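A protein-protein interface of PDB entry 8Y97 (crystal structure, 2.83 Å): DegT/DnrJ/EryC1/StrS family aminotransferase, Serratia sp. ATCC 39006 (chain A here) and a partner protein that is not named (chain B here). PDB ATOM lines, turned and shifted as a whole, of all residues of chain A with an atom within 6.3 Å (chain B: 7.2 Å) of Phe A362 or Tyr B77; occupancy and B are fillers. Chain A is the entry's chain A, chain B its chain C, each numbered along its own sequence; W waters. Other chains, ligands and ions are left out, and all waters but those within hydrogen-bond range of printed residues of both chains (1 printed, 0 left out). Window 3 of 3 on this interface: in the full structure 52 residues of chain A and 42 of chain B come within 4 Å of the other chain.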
ATOM      1  N   LYS A 122     -15.437 -23.322   3.333  1.00  0.00           N
ATOM      2  CA  LYS A 122     -16.310 -24.181   4.119  1.00  0.00           C
ATOM      3  C   LYS A 122     -15.600 -25.498   4.434  1.00  0.00           C
ATOM      4  O   LYS A 122     -16.250 -26.524   4.638  1.00  0.00           O
ATOM      5  CB  LYS A 122     -17.654 -24.394   3.411  1.00  0.00           C
ATOM      6  CG  LYS A 122     -18.391 -23.141   2.946  1.00  0.00           C
ATOM      7  CD  LYS A 122     -19.545 -23.497   2.010  1.00  0.00           C
ATOM      8  CE  LYS A 122     -20.192 -22.329   1.337  1.00  0.00           C
ATOM      9  NZ  LYS A 122     -21.078 -21.591   2.241  1.00  0.00           N
ATOM     10  N   ILE A 124     -12.246 -27.551   6.689  1.00  0.00           N
ATOM     11  CA  ILE A 124     -11.730 -27.592   8.049  1.00  0.00           C
ATOM     12  C   ILE A 124     -10.201 -27.632   8.003  1.00  0.00           C
ATOM     13  O   ILE A 124      -9.614 -28.576   7.476  1.00  0.00           O
ATOM     14  CB  ILE A 124     -12.315 -28.788   8.824  1.00  0.00           C
ATOM     15  CG1 ILE A 124     -13.839 -28.852   8.679  1.00  0.00           C
ATOM     16  CG2 ILE A 124     -11.880 -28.749  10.293  1.00  0.00           C
ATOM     17  CD1 ILE A 124     -14.504 -29.971   9.457  1.00  0.00           C
ATOM     18  N   PHE A 355     -18.933 -19.379   9.896  1.00  0.00           N
ATOM     19  CA  PHE A 355     -20.035 -18.610   9.341  1.00  0.00           C
ATOM     20  C   PHE A 355     -21.092 -18.354  10.412  1.00  0.00           C
ATOM     21  O   PHE A 355     -21.938 -17.476  10.247  1.00  0.00           O
ATOM     22  CB  PHE A 355     -20.680 -19.349   8.167  1.00  0.00           C
ATOM     23  CG  PHE A 355     -19.849 -19.410   6.893  1.00  0.00           C
ATOM     24  CD1 PHE A 355     -18.805 -20.319   6.767  1.00  0.00           C
ATOM     25  CD2 PHE A 355     -20.131 -18.575   5.816  1.00  0.00           C
ATOM     26  CE1 PHE A 355     -18.058 -20.383   5.601  1.00  0.00           C
ATOM     27  CE2 PHE A 355     -19.380 -18.641   4.653  1.00  0.00           C
ATOM     28  CZ  PHE A 355     -18.347 -19.547   4.547  1.00  0.00           C
ATOM     29  N   GLY A 356     -21.048 -19.149  11.488  1.00  0.00           N
ATOM     30  CA  GLY A 356     -22.044 -19.105  12.547  1.00  0.00           C
ATOM     31  C   GLY A 356     -22.402 -20.520  12.997  1.00  0.00           C
ATOM     32  O   GLY A 356     -22.453 -21.436  12.176  1.00  0.00           O
ATOM     33  N   LYS A 357     -22.621 -20.685  14.309  1.00  0.00           N
ATOM     34  CA  LYS A 357     -22.951 -21.973  14.905  1.00  0.00           C
ATOM     35  C   LYS A 357     -21.823 -22.978  14.666  1.00  0.00           C
ATOM     36  O   LYS A 357     -22.030 -24.178  14.821  1.00  0.00           O
ATOM     37  CB  LYS A 357     -24.276 -22.513  14.348  1.00  0.00           C
ATOM     38  CG  LYS A 357     -25.395 -21.483  14.166  1.00  0.00           C
ATOM     39  CD  LYS A 357     -25.877 -20.823  15.455  1.00  0.00           C
ATOM     40  CE  LYS A 357     -26.625 -19.540  15.239  1.00  0.00           C
ATOM     41  NZ  LYS A 357     -27.743 -19.681  14.303  1.00  0.00           N
ATOM     42  N   GLY A 358     -20.634 -22.478  14.303  1.00  0.00           N
ATOM     43  CA  GLY A 358     -19.497 -23.314  13.953  1.00  0.00           C
ATOM     44  C   GLY A 358     -19.714 -24.089  12.656  1.00  0.00           C
ATOM     45  O   GLY A 358     -19.369 -25.266  12.595  1.00  0.00           O
ATOM     46  N   TYR A 359     -20.232 -23.411  11.619  1.00  0.00           N
ATOM     47  CA  TYR A 359     -20.751 -24.087  10.437  1.00  0.00           C
ATOM     48  C   TYR A 359     -19.717 -25.071   9.891  1.00  0.00           C
ATOM     49  O   TYR A 359     -19.996 -26.267   9.823  1.00  0.00           O
ATOM     50  CB  TYR A 359     -21.212 -23.184   9.287  1.00  0.00           C
ATOM     51  CG  TYR A 359     -21.332 -23.919   7.956  1.00  0.00           C
ATOM     52  CD1 TYR A 359     -21.925 -25.176   7.875  1.00  0.00           C
ATOM     53  CD2 TYR A 359     -20.808 -23.378   6.786  1.00  0.00           C
ATOM     54  CE1 TYR A 359     -22.010 -25.861   6.674  1.00  0.00           C
ATOM     55  CE2 TYR A 359     -20.899 -24.048   5.575  1.00  0.00           C
ATOM     56  CZ  TYR A 359     -21.503 -25.292   5.521  1.00  0.00           C
ATOM     57  OH  TYR A 359     -21.607 -25.973   4.344  1.00  0.00           O
ATOM     58  N   PRO A 360     -18.509 -24.634   9.464  1.00  0.00           N
ATOM     59  CA  PRO A 360     -17.560 -25.557   8.837  1.00  0.00           C
ATOM     60  C   PRO A 360     -17.102 -26.658   9.793  1.00  0.00           C
ATOM     61  O   PRO A 360     -16.944 -27.802   9.383  1.00  0.00           O
ATOM     62  CB  PRO A 360     -16.404 -24.640   8.401  1.00  0.00           C
ATOM     63  CG  PRO A 360     -17.006 -23.253   8.413  1.00  0.00           C
ATOM     64  CD  PRO A 360     -17.974 -23.270   9.580  1.00  0.00           C
ATOM     65  N   PHE A 361     -16.939 -26.304  11.073  1.00  0.00           N
ATOM     66  CA  PHE A 361     -16.201 -27.122  12.023  1.00  0.00           C
ATOM     67  C   PHE A 361     -17.028 -28.325  12.480  1.00  0.00           C
ATOM     68  O   PHE A 361     -16.469 -29.404  12.681  1.00  0.00           O
ATOM     69  CB  PHE A 361     -15.761 -26.254  13.206  1.00  0.00           C
ATOM     70  CG  PHE A 361     -14.921 -25.043  12.820  1.00  0.00           C
ATOM     71  CD1 PHE A 361     -13.563 -25.175  12.542  1.00  0.00           C
ATOM     72  CD2 PHE A 361     -15.486 -23.774  12.746  1.00  0.00           C
ATOM     73  CE1 PHE A 361     -12.797 -24.070  12.195  1.00  0.00           C
ATOM     74  CE2 PHE A 361     -14.715 -22.673  12.403  1.00  0.00           C
ATOM     75  CZ  PHE A 361     -13.375 -22.823  12.125  1.00  0.00           C
ATOM     76  N   PHE A 362     -18.349 -28.142  12.641  1.00  0.00           N
ATOM     77  CA  PHE A 362     -19.208 -29.204  13.153  1.00  0.00           C
ATOM     78  C   PHE A 362     -19.423 -30.273  12.078  1.00  0.00           C
ATOM     79  O   PHE A 362     -19.960 -31.340  12.361  1.00  0.00           O
ATOM     80  CB  PHE A 362     -20.521 -28.639  13.717  1.00  0.00           C
ATOM     81  CG  PHE A 362     -21.504 -27.963  12.765  1.00  0.00           C
ATOM     82  CD1 PHE A 362     -21.813 -28.501  11.516  1.00  0.00           C
ATOM     83  CD2 PHE A 362     -22.149 -26.790  13.141  1.00  0.00           C
ATOM     84  CE1 PHE A 362     -22.720 -27.876  10.672  1.00  0.00           C
ATOM     85  CE2 PHE A 362     -23.057 -26.170  12.296  1.00  0.00           C
ATOM     86  CZ  PHE A 362     -23.341 -26.713  11.064  1.00  0.00           C
ATOM     87  N   LEU A 363     -18.989 -29.973  10.845  1.00  0.00           N
ATOM     88  CA  LEU A 363     -19.150 -30.854   9.702  1.00  0.00           C
ATOM     89  C   LEU A 363     -17.971 -31.829   9.649  1.00  0.00           C
ATOM     90  O   LEU A 363     -17.638 -32.330   8.574  1.00  0.00           O
ATOM     91  CB  LEU A 363     -19.224 -29.945   8.472  1.00  0.00           C
ATOM     92  CG  LEU A 363     -20.266 -30.309   7.411  1.00  0.00           C
ATOM     93  CD1 LEU A 363     -21.662 -30.346   8.011  1.00  0.00           C
ATOM     94  CD2 LEU A 363     -20.195 -29.310   6.268  1.00  0.00           C
ATOM     95  N   GLY A 364     -17.340 -32.099  10.801  1.00  0.00           N
ATOM     96  CA  GLY A 364     -16.249 -33.056  10.891  1.00  0.00           C
ATOM     97  C   GLY A 364     -15.761 -33.195  12.334  1.00  0.00           C
ATOM     98  O   GLY A 364     -16.165 -32.436  13.214  1.00  0.00           O
ATOM     99  N   ASP A 365     -14.862 -34.161  12.551  1.00  0.00           N
ATOM    100  CA  ASP A 365     -14.413 -34.545  13.882  1.00  0.00           C
ATOM    101  C   ASP A 365     -13.682 -33.385  14.556  1.00  0.00           C
ATOM    102  O   ASP A 365     -12.664 -32.915  14.051  1.00  0.00           O
ATOM    103  CB  ASP A 365     -13.518 -35.776  13.830  1.00  0.00           C
ATOM    104  CG  ASP A 365     -14.179 -37.063  13.349  1.00  0.00           C
ATOM    105  OD1 ASP A 365     -14.860 -37.014  12.305  1.00  0.00           O
ATOM    106  OD2 ASP A 365     -13.985 -38.112  14.007  1.00  0.00           O
ATOM    107  N   TRP B  71     -23.852  -9.955   9.964  1.00  0.00           N
ATOM    108  CA  TRP B  71     -23.154 -10.498  11.121  1.00  0.00           C
ATOM    109  C   TRP B  71     -23.154  -9.500  12.277  1.00  0.00           C
ATOM    110  O   TRP B  71     -23.056  -9.898  13.435  1.00  0.00           O
ATOM    111  CB  TRP B  71     -21.719 -10.886  10.737  1.00  0.00           C
ATOM    112  CG  TRP B  71     -21.620 -12.120   9.880  1.00  0.00           C
ATOM    113  CD1 TRP B  71     -22.640 -12.810   9.293  1.00  0.00           C
ATOM    114  CD2 TRP B  71     -20.405 -12.799   9.495  1.00  0.00           C
ATOM    115  NE1 TRP B  71     -22.151 -13.879   8.591  1.00  0.00           N
ATOM    116  CE2 TRP B  71     -20.786 -13.895   8.689  1.00  0.00           C
ATOM    117  CE3 TRP B  71     -19.047 -12.590   9.754  1.00  0.00           C
ATOM    118  CZ2 TRP B  71     -19.852 -14.774   8.145  1.00  0.00           C
ATOM    119  CZ3 TRP B  71     -18.125 -13.460   9.214  1.00  0.00           C
ATOM    120  CH2 TRP B  71     -18.525 -14.535   8.421  1.00  0.00           C
ATOM    121  N   ASP B  74     -26.090 -10.191  14.260  1.00  0.00           N
ATOM    122  CA  ASP B  74     -26.131 -11.607  14.594  1.00  0.00           C
ATOM    123  C   ASP B  74     -26.989 -12.393  13.601  1.00  0.00           C
ATOM    124  O   ASP B  74     -27.535 -13.434  13.956  1.00  0.00           O
ATOM    125  CB  ASP B  74     -26.567 -11.828  16.036  1.00  0.00           C
ATOM    126  CG  ASP B  74     -25.617 -11.279  17.090  1.00  0.00           C
ATOM    127  OD1 ASP B  74     -24.488 -11.800  17.191  1.00  0.00           O
ATOM    128  OD2 ASP B  74     -26.005 -10.321  17.789  1.00  0.00           O
ATOM    129  N   ILE B  75     -27.082 -11.911  12.353  1.00  0.00           N
ATOM    130  CA  ILE B  75     -27.742 -12.651  11.291  1.00  0.00           C
ATOM    131  C   ILE B  75     -26.686 -13.526  10.617  1.00  0.00           C
ATOM    132  O   ILE B  75     -26.072 -13.119   9.631  1.00  0.00           O
ATOM    133  CB  ILE B  75     -28.449 -11.708  10.297  1.00  0.00           C
ATOM    134  CG1 ILE B  75     -29.369 -10.712  11.022  1.00  0.00           C
ATOM    135  CG2 ILE B  75     -29.205 -12.508   9.230  1.00  0.00           C
ATOM    136  CD1 ILE B  75     -30.034  -9.689  10.117  1.00  0.00           C
ATOM    137  N   VAL B  76     -26.483 -14.724  11.177  1.00  0.00           N
ATOM    138  CA  VAL B  76     -25.389 -15.602  10.791  1.00  0.00           C
ATOM    139  C   VAL B  76     -25.971 -16.884  10.199  1.00  0.00           C
ATOM    140  O   VAL B  76     -27.163 -16.949   9.914  1.00  0.00           O
ATOM    141  CB  VAL B  76     -24.470 -15.876  12.001  1.00  0.00           C
ATOM    142  CG1 VAL B  76     -23.883 -14.590  12.567  1.00  0.00           C
ATOM    143  CG2 VAL B  76     -25.172 -16.663  13.102  1.00  0.00           C
ATOM    144  N   TYR B  77     -25.111 -17.889   9.995  1.00  0.00           N
ATOM    145  CA  TYR B  77     -25.524 -19.184   9.475  1.00  0.00           C
ATOM    146  C   TYR B  77     -26.648 -19.752  10.340  1.00  0.00           C
ATOM    147  O   TYR B  77     -26.481 -19.903  11.548  1.00  0.00           O
ATOM    148  CB  TYR B  77     -24.305 -20.114   9.444  1.00  0.00           C
ATOM    149  CG  TYR B  77     -24.568 -21.507   8.885  1.00  0.00           C
ATOM    150  CD1 TYR B  77     -25.007 -22.544   9.701  1.00  0.00           C
ATOM    151  CD2 TYR B  77     -24.362 -21.784   7.538  1.00  0.00           C
ATOM    152  CE1 TYR B  77     -25.245 -23.811   9.191  1.00  0.00           C
ATOM    153  CE2 TYR B  77     -24.596 -23.046   7.016  1.00  0.00           C
ATOM    154  CZ  TYR B  77     -25.039 -24.063   7.844  1.00  0.00           C
ATOM    155  OH  TYR B  77     -25.267 -25.308   7.333  1.00  0.00           O
ATOM    156  N   GLY B  78     -27.790 -20.053   9.707  1.00  0.00           N
ATOM    157  CA  GLY B  78     -28.921 -20.661  10.391  1.00  0.00           C
ATOM    158  C   GLY B  78     -30.042 -19.661  10.669  1.00  0.00           C
ATOM    159  O   GLY B  78     -31.187 -20.063  10.858  1.00  0.00           O
ATOM    160  N   GLU B  79     -29.703 -18.364  10.701  1.00  0.00           N
ATOM    161  CA  GLU B  79     -30.676 -17.309  10.943  1.00  0.00           C
ATOM    162  C   GLU B  79     -31.360 -16.928   9.630  1.00  0.00           C
ATOM    163  O   GLU B  79     -31.060 -17.495   8.580  1.00  0.00           O
ATOM    164  CB  GLU B  79     -29.982 -16.107  11.585  1.00  0.00           C
ATOM    165  CG  GLU B  79     -29.339 -16.434  12.929  1.00  0.00           C
ATOM    166  CD  GLU B  79     -30.316 -16.778  14.039  1.00  0.00           C
ATOM    167  OE1 GLU B  79     -31.467 -16.288  14.042  1.00  0.00           O
ATOM    168  OE2 GLU B  79     -29.912 -17.574  14.905  1.00  0.00           O
ATOM    169  N   ALA B  80     -32.293 -15.970   9.710  1.00  0.00           N
ATOM    170  CA  ALA B  80     -33.024 -15.494   8.547  1.00  0.00           C
ATOM    171  C   ALA B  80     -33.278 -13.996   8.666  1.00  0.00           C
ATOM    172  O   ALA B  80     -33.131 -13.417   9.742  1.00  0.00           O
ATOM    173  CB  ALA B  80     -34.320 -16.260   8.410  1.00  0.00           C
ATOM    174  N   LYS B  95     -27.541 -16.775   0.513  1.00  0.00           N
ATOM    175  CA  LYS B  95     -27.636 -18.226   0.432  1.00  0.00           C
ATOM    176  C   LYS B  95     -26.293 -18.864   0.781  1.00  0.00           C
ATOM    177  O   LYS B  95     -26.253 -19.889   1.458  1.00  0.00           O
ATOM    178  CB  LYS B  95     -28.090 -18.668  -0.964  1.00  0.00           C
ATOM    179  CG  LYS B  95     -28.158 -20.177  -1.170  1.00  0.00           C
ATOM    180  CD  LYS B  95     -28.586 -20.598  -2.570  1.00  0.00           C
ATOM    181  CE  LYS B  95     -28.448 -22.073  -2.788  1.00  0.00           C
ATOM    182  NZ  LYS B  95     -28.661 -22.439  -4.190  1.00  0.00           N
ATOM    183  N   TRP B  96     -25.203 -18.251   0.305  1.00  0.00           N
ATOM    184  CA  TRP B  96     -23.858 -18.747   0.550  1.00  0.00           C
ATOM    185  C   TRP B  96     -23.504 -18.619   2.031  1.00  0.00           C
ATOM    186  O   TRP B  96     -22.833 -19.490   2.581  1.00  0.00           O
ATOM    187  CB  TRP B  96     -22.854 -18.003  -0.341  1.00  0.00           C
ATOM    188  CG  TRP B  96     -21.415 -18.367  -0.089  1.00  0.00           C
ATOM    189  CD1 TRP B  96     -20.755 -19.467  -0.548  1.00  0.00           C
ATOM    190  CD2 TRP B  96     -20.454 -17.614   0.682  1.00  0.00           C
ATOM    191  NE1 TRP B  96     -19.453 -19.454  -0.121  1.00  0.00           N
ATOM    192  CE2 TRP B  96     -19.239 -18.331   0.635  1.00  0.00           C
ATOM    193  CE3 TRP B  96     -20.498 -16.413   1.397  1.00  0.00           C
ATOM    194  CZ2 TRP B  96     -18.088 -17.884   1.279  1.00  0.00           C
ATOM    195  CZ3 TRP B  96     -19.358 -15.972   2.034  1.00  0.00           C
ATOM    196  CH2 TRP B  96     -18.170 -16.699   1.972  1.00  0.00           C
ATOM    197  N   LEU B  97     -23.967 -17.533   2.667  1.00  0.00           N
ATOM    198  CA  LEU B  97     -23.755 -17.305   4.088  1.00  0.00           C
ATOM    199  C   LEU B  97     -24.611 -18.260   4.917  1.00  0.00           C
ATOM    200  O   LEU B  97     -24.321 -18.475   6.093  1.00  0.00           O
ATOM    201  CB  LEU B  97     -24.073 -15.851   4.436  1.00  0.00           C
ATOM    202  CG  LEU B  97     -23.068 -14.801   3.957  1.00  0.00           C
ATOM    203  CD1 LEU B  97     -23.659 -13.407   4.055  1.00  0.00           C
ATOM    204  CD2 LEU B  97     -21.775 -14.879   4.748  1.00  0.00           C
ATOM    205  N   GLY B  98     -25.678 -18.795   4.308  1.00  0.00           N
ATOM    206  CA  GLY B  98     -26.583 -19.718   4.975  1.00  0.00           C
ATOM    207  C   GLY B  98     -27.669 -18.970   5.748  1.00  0.00           C
ATOM    208  O   GLY B  98     -27.958 -19.298   6.897  1.00  0.00           O
ATOM    209  N   ILE B  99     -28.262 -17.968   5.089  1.00  0.00           N
ATOM    210  CA  ILE B  99     -29.271 -17.112   5.689  1.00  0.00           C
ATOM    211  C   ILE B  99     -30.552 -17.225   4.863  1.00  0.00           C
ATOM    212  O   ILE B  99     -30.514 -17.100   3.640  1.00  0.00           O
ATOM    213  CB  ILE B  99     -28.761 -15.660   5.784  1.00  0.00           C
ATOM    214  CG1 ILE B  99     -27.567 -15.552   6.742  1.00  0.00           C
ATOM    215  CG2 ILE B  99     -29.887 -14.698   6.174  1.00  0.00           C
ATOM    216  CD1 ILE B  99     -26.795 -14.248   6.634  1.00  0.00           C
HETATM  217  O   HOH W   1     -22.940 -16.668   7.679  1.00  0.00           O
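Among the printed residues, pairs that only touch across the chains: Phe A355 with Trp B71 (3.97 Å), Phe A355 with Val B76 (3.5 Å), Phe A355 with Trp B96 (3.5 Å), Gly A356 with Tyr B77 (3.6 Å), Lys A357 with Val B76 (3.9 Å), Tyr A359 with Tyr B77 (3.3 Å) and Phe A362 with Tyr B77 (3.9 Å).
Of the 13 printed residues of chain A, 6 touch a printed residue of chain B.
Printed residues of chain A that touch a printed residue of chain B: Lys A122, Phe A355, Gly A356, Lys A357, Tyr A359 and Phe A362.
Hydrophobic or aromatic side chains of chain A within 4 Å of the printed part of chain B: Phe A355, Tyr A359 and Phe A362.
Among the printed residues, Asp or Glu carboxylates within 4 Å of a Lys or Arg side-chain nitrogen of the other chain: Lys A357 with Glu B79.
NZ of Lys A357 is in salt-bridge range of OE2 of Glu B79 (3.1 Å).
The backbone carbonyl oxygen of Phe A355 is in hydrogen-bond range of the backbone NH of Tyr B77 (3.2 Å).
NZ of Lys A357 sits at hydrogen-bond distance from O of Tyr B77 (3.0 Å).
The side-chain amino group (NZ) of Lys A122 lies within hydrogen-bond range of the backbone carbonyl oxygen (O) of Trp B96 (2.8 Å).
Of chain A, only Phe A355, Gly A356, Lys A357, Tyr A359 and Phe A362 come within 4 Å of Tyr B77.
Printed residues of chain A within 4 Å of Val B76: Phe A355 (3.5 Å) and Lys A357 (3.9 Å).
Of the printed residues of chain B, Phe A355 touches Trp B71 (3.97 Å), Val B76 (3.5 Å), Tyr B77 (3.2 Å) and Trp B96 (3.5 Å).
Water W1 lies within hydrogen-bond range of O of Leu B97, O of Phe A355, NE1 of Trp B71 and N of Tyr B77.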
